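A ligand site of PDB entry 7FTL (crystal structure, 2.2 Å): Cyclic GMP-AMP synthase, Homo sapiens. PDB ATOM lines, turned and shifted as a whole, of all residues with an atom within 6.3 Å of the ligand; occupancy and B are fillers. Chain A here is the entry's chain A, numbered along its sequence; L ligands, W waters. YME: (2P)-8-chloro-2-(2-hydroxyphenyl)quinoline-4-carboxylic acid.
Water W1 lies within hydrogen-bond range of O11 of the ligand (2.6 Å), OH of Tyr 276 (2.6 Å) and OE2 of Glu 223 (2.7 Å).
The backbone carbonyl oxygen (O) of Phe 328 sits at hydrogen-bond distance from the backbone NH (N) of Asn 322 (3.0 Å).
The side-chain hydroxyl of Tyr 276 is in hydrogen-bond range of the side-chain amide nitrogen of Asn 322 (3.0 Å).
N of Ile 325 sits at hydrogen-bond distance from OD1 of Asn 322 (3.0 Å).
The side-chain amide oxygen of Asn 322 lies within hydrogen-bond range of the backbone NH of Phe 324 (2.8 Å).
NH1 of Arg 216 lies within hydrogen-bond range of OH of Tyr 88, 3.1 Å away.
The backbone NH (N) of Arg 216 lies within hydrogen-bond range of the backbone carbonyl oxygen (O) of Val 200.
N of Leu 217 is in hydrogen-bond range of O of Ala 87, 3.3 Å away.
The backbone NH (N) of Ser 274 is in hydrogen-bond range of a ring nitrogen (ND1) of His 277 (3.0 Å).
The side-chain hydroxyl of Ser 218 is in hydrogen-bond range of an oxygen (O12) of the ligand (2.5 Å).
The backbone NH of Ser 220 lies within hydrogen-bond range of an oxygen (O11) of the ligand (3.3 Å).
An oxygen (O12) of the ligand sits at hydrogen-bond distance from the side-chain hydroxyl (OG) of Ser 220, at 2.9 Å.
The backbone NH (N) of Phe 219 lies within hydrogen-bond range of an oxygen (O11) of the ligand, at 2.9 Å.
The guanidinium group (NH1) of Arg 216 sits at hydrogen-bond distance from an oxygen (O14) of the ligand (3.3 Å).
Merely in contact with the ligand: Ala 87 (3.6 Å), Leu 217 (3.7 Å), Ser 274 (3.9 Å), Tyr 276 (3.5 Å), Asn 322 (3.2 Å), Phe 328 (3.4 Å) and Leu 330 (3.6 Å).
Hydrophobic or aromatic side chains that line the ligand: Ala 87, Tyr 276, Phe 328 and Leu 330.
11 residues have an atom within 4 Å of the ligand: Ala 87, Arg 216, Leu 217, Ser 218, Phe 219, Ser 220, Ser 274, Tyr 276, Asn 322, Phe 328 and Leu 330.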
ATOM      1  N   VAL A  58      11.324  30.138  20.631  1.00  0.00           N
ATOM      2  CA  VAL A  58      12.742  30.328  20.910  1.00  0.00           C
ATOM      3  C   VAL A  58      13.049  31.805  21.133  1.00  0.00           C
ATOM      4  O   VAL A  58      13.611  32.198  22.165  1.00  0.00           O
ATOM      5  CB  VAL A  58      13.599  29.760  19.767  1.00  0.00           C
ATOM      6  CG1 VAL A  58      15.038  30.215  19.910  1.00  0.00           C
ATOM      7  CG2 VAL A  58      13.511  28.232  19.756  1.00  0.00           C
ATOM      8  N   MET A  69       8.611  21.257  15.075  1.00  0.00           N
ATOM      9  CA  MET A  69       9.480  20.174  14.632  1.00  0.00           C
ATOM     10  C   MET A  69       8.636  18.964  14.266  1.00  0.00           C
ATOM     11  O   MET A  69       7.825  18.517  15.077  1.00  0.00           O
ATOM     12  CB  MET A  69      10.512  19.799  15.710  1.00  0.00           C
ATOM     13  CG  MET A  69      11.278  18.528  15.400  1.00  0.00           C
ATOM     14  SD  MET A  69      12.690  18.286  16.488  1.00  0.00           S
ATOM     15  CE  MET A  69      13.706  19.697  16.040  1.00  0.00           C
ATOM     16  N   ALA A  87      29.464  15.960  16.620  1.00  0.00           N
ATOM     17  CA  ALA A  87      28.044  16.314  16.538  1.00  0.00           C
ATOM     18  C   ALA A  87      27.409  16.060  15.175  1.00  0.00           C
ATOM     19  O   ALA A  87      26.180  15.974  15.113  1.00  0.00           O
ATOM     20  CB  ALA A  87      27.847  17.796  16.888  1.00  0.00           C
ATOM     21  N   TYR A  88      28.184  15.937  14.099  1.00  0.00           N
ATOM     22  CA  TYR A  88      27.644  15.743  12.762  1.00  0.00           C
ATOM     23  C   TYR A  88      27.891  14.315  12.315  1.00  0.00           C
ATOM     24  O   TYR A  88      28.990  13.777  12.480  1.00  0.00           O
ATOM     25  CB  TYR A  88      28.273  16.733  11.775  1.00  0.00           C
ATOM     26  CG  TYR A  88      27.883  18.171  12.071  1.00  0.00           C
ATOM     27  CD1 TYR A  88      26.764  18.735  11.470  1.00  0.00           C
ATOM     28  CD2 TYR A  88      28.626  18.943  12.957  1.00  0.00           C
ATOM     29  CE1 TYR A  88      26.406  20.041  11.741  1.00  0.00           C
ATOM     30  CE2 TYR A  88      28.259  20.252  13.231  1.00  0.00           C
ATOM     31  CZ  TYR A  88      27.149  20.790  12.618  1.00  0.00           C
ATOM     32  OH  TYR A  88      26.788  22.090  12.882  1.00  0.00           O
ATOM     33  N   VAL A 200      18.822  16.402  12.827  1.00  0.00           N
ATOM     34  CA  VAL A 200      18.301  17.371  11.865  1.00  0.00           C
ATOM     35  C   VAL A 200      19.352  17.612  10.784  1.00  0.00           C
ATOM     36  O   VAL A 200      20.558  17.497  11.056  1.00  0.00           O
ATOM     37  CB  VAL A 200      17.887  18.689  12.556  1.00  0.00           C
ATOM     38  CG1 VAL A 200      16.959  18.403  13.716  1.00  0.00           C
ATOM     39  CG2 VAL A 200      19.108  19.468  13.016  1.00  0.00           C
ATOM     40  N   ARG A 216      22.817  16.635  12.521  1.00  0.00           N
ATOM     41  CA  ARG A 216      23.289  17.124  13.802  1.00  0.00           C
ATOM     42  C   ARG A 216      22.395  16.600  14.924  1.00  0.00           C
ATOM     43  O   ARG A 216      21.169  16.548  14.778  1.00  0.00           O
ATOM     44  CB  ARG A 216      23.333  18.660  13.844  1.00  0.00           C
ATOM     45  CG  ARG A 216      23.969  19.223  15.102  1.00  0.00           C
ATOM     46  CD  ARG A 216      24.384  20.667  14.921  1.00  0.00           C
ATOM     47  NE  ARG A 216      23.249  21.586  14.973  1.00  0.00           N
ATOM     48  CZ  ARG A 216      23.341  22.891  14.757  1.00  0.00           C
ATOM     49  NH1 ARG A 216      24.496  23.466  14.448  1.00  0.00           N
ATOM     50  NH2 ARG A 216      22.249  23.641  14.837  1.00  0.00           N
ATOM     51  N   LEU A 217      23.021  16.227  16.038  1.00  0.00           N
ATOM     52  CA  LEU A 217      22.282  15.747  17.194  1.00  0.00           C
ATOM     53  C   LEU A 217      21.474  16.872  17.820  1.00  0.00           C
ATOM     54  O   LEU A 217      21.929  18.028  17.884  1.00  0.00           O
ATOM     55  CB  LEU A 217      23.236  15.153  18.237  1.00  0.00           C
ATOM     56  CG  LEU A 217      24.149  13.999  17.812  1.00  0.00           C
ATOM     57  CD1 LEU A 217      25.104  13.629  18.928  1.00  0.00           C
ATOM     58  CD2 LEU A 217      23.334  12.789  17.390  1.00  0.00           C
ATOM     59  N   SER A 218      20.263  16.553  18.276  1.00  0.00           N
ATOM     60  CA  SER A 218      19.359  17.519  18.885  1.00  0.00           C
ATOM     61  C   SER A 218      18.805  16.944  20.181  1.00  0.00           C
ATOM     62  O   SER A 218      18.272  15.829  20.181  1.00  0.00           O
ATOM     63  CB  SER A 218      18.220  17.882  17.927  1.00  0.00           C
ATOM     64  OG  SER A 218      17.291  18.743  18.549  1.00  0.00           O
ATOM     65  N   PHE A 219      18.927  17.708  21.268  1.00  0.00           N
ATOM     66  CA  PHE A 219      18.439  17.297  22.580  1.00  0.00           C
ATOM     67  C   PHE A 219      17.556  18.375  23.200  1.00  0.00           C
ATOM     68  O   PHE A 219      17.465  18.469  24.429  1.00  0.00           O
ATOM     69  CB  PHE A 219      19.595  16.966  23.517  1.00  0.00           C
ATOM     70  CG  PHE A 219      20.504  15.886  23.008  1.00  0.00           C
ATOM     71  CD1 PHE A 219      20.166  14.551  23.159  1.00  0.00           C
ATOM     72  CD2 PHE A 219      21.710  16.200  22.407  1.00  0.00           C
ATOM     73  CE1 PHE A 219      21.005  13.549  22.696  1.00  0.00           C
ATOM     74  CE2 PHE A 219      22.563  15.208  21.943  1.00  0.00           C
ATOM     75  CZ  PHE A 219      22.204  13.881  22.084  1.00  0.00           C
ATOM     76  N   SER A 220      16.903  19.197  22.368  1.00  0.00           N
ATOM     77  CA  SER A 220      16.046  20.256  22.893  1.00  0.00           C
ATOM     78  C   SER A 220      14.916  19.686  23.750  1.00  0.00           C
ATOM     79  O   SER A 220      14.492  20.325  24.717  1.00  0.00           O
ATOM     80  CB  SER A 220      15.478  21.079  21.740  1.00  0.00           C
ATOM     81  OG  SER A 220      16.516  21.744  21.037  1.00  0.00           O
ATOM     82  N   HIS A 221      14.426  18.497  23.413  1.00  0.00           N
ATOM     83  CA  HIS A 221      13.402  17.851  24.232  1.00  0.00           C
ATOM     84  C   HIS A 221      13.928  17.531  25.620  1.00  0.00           C
ATOM     85  O   HIS A 221      13.159  17.590  26.591  1.00  0.00           O
ATOM     86  CB  HIS A 221      12.912  16.577  23.534  1.00  0.00           C
ATOM     87  CG  HIS A 221      13.984  15.562  23.329  1.00  0.00           C
ATOM     88  ND1 HIS A 221      15.042  15.765  22.466  1.00  0.00           N
ATOM     89  CD2 HIS A 221      14.173  14.336  23.856  1.00  0.00           C
ATOM     90  CE1 HIS A 221      15.836  14.708  22.484  1.00  0.00           C
ATOM     91  NE2 HIS A 221      15.330  13.823  23.323  1.00  0.00           N
ATOM     92  N   GLU A 223      16.310  19.314  27.112  1.00  0.00           N
ATOM     93  CA  GLU A 223      16.428  20.620  27.763  1.00  0.00           C
ATOM     94  C   GLU A 223      15.075  21.096  28.265  1.00  0.00           C
ATOM     95  O   GLU A 223      14.974  21.664  29.362  1.00  0.00           O
ATOM     96  CB  GLU A 223      17.047  21.628  26.795  1.00  0.00           C
ATOM     97  CG  GLU A 223      18.423  21.241  26.294  1.00  0.00           C
ATOM     98  CD  GLU A 223      18.828  22.042  25.079  1.00  0.00           C
ATOM     99  OE1 GLU A 223      18.034  22.890  24.619  1.00  0.00           O
ATOM    100  OE2 GLU A 223      19.948  21.831  24.563  1.00  0.00           O
ATOM    101  N   SER A 274      23.204  32.922  18.994  1.00  0.00           N
ATOM    102  CA  SER A 274      21.785  32.597  19.097  1.00  0.00           C
ATOM    103  C   SER A 274      21.464  32.281  20.549  1.00  0.00           C
ATOM    104  O   SER A 274      22.358  32.184  21.401  1.00  0.00           O
ATOM    105  CB  SER A 274      21.421  31.415  18.191  1.00  0.00           C
ATOM    106  OG  SER A 274      22.101  30.235  18.600  1.00  0.00           O
ATOM    107  N   SER A 275      20.180  32.114  20.829  1.00  0.00           N
ATOM    108  CA  SER A 275      19.745  31.817  22.189  1.00  0.00           C
ATOM    109  C   SER A 275      20.303  30.489  22.682  1.00  0.00           C
ATOM    110  O   SER A 275      20.386  30.266  23.900  1.00  0.00           O
ATOM    111  CB  SER A 275      18.222  31.814  22.275  1.00  0.00           C
ATOM    112  OG  SER A 275      17.687  30.658  21.660  1.00  0.00           O
ATOM    113  N   TYR A 276      20.691  29.603  21.763  1.00  0.00           N
ATOM    114  CA  TYR A 276      21.253  28.317  22.166  1.00  0.00           C
ATOM    115  C   TYR A 276      22.588  28.490  22.887  1.00  0.00           C
ATOM    116  O   TYR A 276      22.894  27.735  23.810  1.00  0.00           O
ATOM    117  CB  TYR A 276      21.417  27.413  20.939  1.00  0.00           C
ATOM    118  CG  TYR A 276      21.913  26.028  21.263  1.00  0.00           C
ATOM    119  CD1 TYR A 276      21.035  25.037  21.681  1.00  0.00           C
ATOM    120  CD2 TYR A 276      23.258  25.705  21.168  1.00  0.00           C
ATOM    121  CE1 TYR A 276      21.475  23.758  21.978  1.00  0.00           C
ATOM    122  CE2 TYR A 276      23.709  24.431  21.456  1.00  0.00           C
ATOM    123  CZ  TYR A 276      22.815  23.461  21.866  1.00  0.00           C
ATOM    124  OH  TYR A 276      23.270  22.192  22.162  1.00  0.00           O
ATOM    125  N   HIS A 277      23.388  29.473  22.476  1.00  0.00           N
ATOM    126  CA  HIS A 277      24.626  29.753  23.180  1.00  0.00           C
ATOM    127  C   HIS A 277      24.349  30.226  24.597  1.00  0.00           C
ATOM    128  O   HIS A 277      24.982  29.769  25.554  1.00  0.00           O
ATOM    129  CB  HIS A 277      25.442  30.803  22.418  1.00  0.00           C
ATOM    130  CG  HIS A 277      25.848  30.384  21.042  1.00  0.00           C
ATOM    131  ND1 HIS A 277      25.143  30.758  19.914  1.00  0.00           N
ATOM    132  CD2 HIS A 277      26.887  29.638  20.602  1.00  0.00           C
ATOM    133  CE1 HIS A 277      25.732  30.251  18.838  1.00  0.00           C
ATOM    134  NE2 HIS A 277      26.790  29.571  19.232  1.00  0.00           N
ATOM    135  N   ASN A 322      29.366  22.310  24.322  1.00  0.00           N
ATOM    136  CA  ASN A 322      28.020  21.790  24.168  1.00  0.00           C
ATOM    137  C   ASN A 322      27.656  20.994  25.412  1.00  0.00           C
ATOM    138  O   ASN A 322      28.424  20.142  25.861  1.00  0.00           O
ATOM    139  CB  ASN A 322      27.918  20.922  22.918  1.00  0.00           C
ATOM    140  CG  ASN A 322      26.504  20.450  22.637  1.00  0.00           C
ATOM    141  OD1 ASN A 322      25.927  19.665  23.394  1.00  0.00           O
ATOM    142  ND2 ASN A 322      25.944  20.911  21.529  1.00  0.00           N
ATOM    143  N   PHE A 324      25.663  18.646  26.013  1.00  0.00           N
ATOM    144  CA  PHE A 324      25.541  17.210  25.811  1.00  0.00           C
ATOM    145  C   PHE A 324      26.774  16.590  25.169  1.00  0.00           C
ATOM    146  O   PHE A 324      26.988  15.378  25.287  1.00  0.00           O
ATOM    147  CB  PHE A 324      24.315  16.888  24.954  1.00  0.00           C
ATOM    148  CG  PHE A 324      23.026  17.397  25.534  1.00  0.00           C
ATOM    149  CD1 PHE A 324      22.610  18.706  25.338  1.00  0.00           C
ATOM    150  CD2 PHE A 324      22.213  16.544  26.278  1.00  0.00           C
ATOM    151  CE1 PHE A 324      21.423  19.162  25.877  1.00  0.00           C
ATOM    152  CE2 PHE A 324      21.022  16.995  26.809  1.00  0.00           C
ATOM    153  CZ  PHE A 324      20.629  18.310  26.609  1.00  0.00           C
ATOM    154  N   ILE A 325      27.591  17.392  24.476  1.00  0.00           N
ATOM    155  CA  ILE A 325      28.774  16.909  23.782  1.00  0.00           C
ATOM    156  C   ILE A 325      29.967  17.751  24.249  1.00  0.00           C
ATOM    157  O   ILE A 325      30.214  18.827  23.675  1.00  0.00           O
ATOM    158  CB  ILE A 325      28.591  16.975  22.257  1.00  0.00           C
ATOM    159  CG1 ILE A 325      27.263  16.310  21.862  1.00  0.00           C
ATOM    160  CG2 ILE A 325      29.756  16.301  21.556  1.00  0.00           C
ATOM    161  CD1 ILE A 325      26.759  16.703  20.501  1.00  0.00           C
ATOM    162  N   PHE A 328      32.652  19.454  21.771  1.00  0.00           N
ATOM    163  CA  PHE A 328      32.238  20.401  20.742  1.00  0.00           C
ATOM    164  C   PHE A 328      32.258  21.800  21.345  1.00  0.00           C
ATOM    165  O   PHE A 328      31.414  22.130  22.185  1.00  0.00           O
ATOM    166  CB  PHE A 328      30.850  20.056  20.197  1.00  0.00           C
ATOM    167  CG  PHE A 328      30.529  20.754  18.899  1.00  0.00           C
ATOM    168  CD1 PHE A 328      30.037  22.050  18.905  1.00  0.00           C
ATOM    169  CD2 PHE A 328      30.722  20.119  17.695  1.00  0.00           C
ATOM    170  CE1 PHE A 328      29.742  22.688  17.710  1.00  0.00           C
ATOM    171  CE2 PHE A 328      30.421  20.743  16.500  1.00  0.00           C
ATOM    172  CZ  PHE A 328      29.937  22.029  16.510  1.00  0.00           C
ATOM    173  N   LEU A 330      31.378  25.342  21.055  1.00  0.00           N
ATOM    174  CA  LEU A 330      30.520  26.261  20.312  1.00  0.00           C
ATOM    175  C   LEU A 330      31.210  27.583  20.011  1.00  0.00           C
ATOM    176  O   LEU A 330      30.797  28.288  19.087  1.00  0.00           O
ATOM    177  CB  LEU A 330      29.220  26.519  21.093  1.00  0.00           C
ATOM    178  CG  LEU A 330      28.388  25.287  21.441  1.00  0.00           C
ATOM    179  CD1 LEU A 330      27.321  25.639  22.452  1.00  0.00           C
ATOM    180  CD2 LEU A 330      27.752  24.684  20.200  1.00  0.00           C
ATOM    181  N   LEU A 335      34.236  28.293  14.160  1.00  0.00           N
ATOM    182  CA  LEU A 335      32.811  28.601  14.130  1.00  0.00           C
ATOM    183  C   LEU A 335      32.553  30.096  14.254  1.00  0.00           C
ATOM    184  O   LEU A 335      31.763  30.657  13.480  1.00  0.00           O
ATOM    185  CB  LEU A 335      32.086  27.852  15.255  1.00  0.00           C
ATOM    186  CG  LEU A 335      32.041  26.327  15.149  1.00  0.00           C
ATOM    187  CD1 LEU A 335      31.306  25.737  16.348  1.00  0.00           C
ATOM    188  CD2 LEU A 335      31.380  25.897  13.855  1.00  0.00           C
HETATM  189  C10 YME L   1      25.042  22.955  17.863  1.00  0.00           C
HETATM  190  O12 YME L   1      18.273  21.036  18.821  1.00  0.00           O
HETATM  191  O14 YME L   1      24.842  24.246  17.593  1.00  0.00           O
HETATM  192  C15 YME L   1      18.752  23.988  18.762  1.00  0.00           C
HETATM  193  C16 YME L   1      24.388  20.736  18.598  1.00  0.00           C
HETATM  194  C17 YME L   1      18.525  25.281  18.381  1.00  0.00           C
HETATM  195  C18 YME L   1      19.590  26.096  17.918  1.00  0.00           C
HETATM  196  C19 YME L   1      26.358  22.505  17.663  1.00  0.00           C
HETATM  197  C20 YME L   1      25.678  20.305  18.398  1.00  0.00           C
HETATM  198  C21 YME L   1      26.665  21.181  17.929  1.00  0.00           C
HETATM  199  C2  YME L   1      22.671  22.518  18.493  1.00  0.00           C
HETATM  200  C3  YME L   1      20.386  22.082  19.077  1.00  0.00           C
HETATM  201  C4  YME L   1      21.121  24.229  18.244  1.00  0.00           C
HETATM  202  C5  YME L   1      20.049  23.424  18.703  1.00  0.00           C
HETATM  203  C6  YME L   1      21.663  21.634  18.980  1.00  0.00           C
HETATM  204  C7  YME L   1      24.042  22.076  18.327  1.00  0.00           C
HETATM  205  C8  YME L   1      19.365  21.154  19.619  1.00  0.00           C
HETATM  206  C9  YME L   1      20.848  25.570  17.864  1.00  0.00           C
HETATM  207  N1  YME L   1      22.416  23.774  18.142  1.00  0.00           N
HETATM  208  O11 YME L   1      19.427  20.516  20.663  1.00  0.00           O
HETATM  209 CL13 YME L   1      22.159  26.537  17.330  1.00  0.00          CL
HETATM  210  O   HOH W   1      21.220  20.594  22.510  1.00  0.00           O
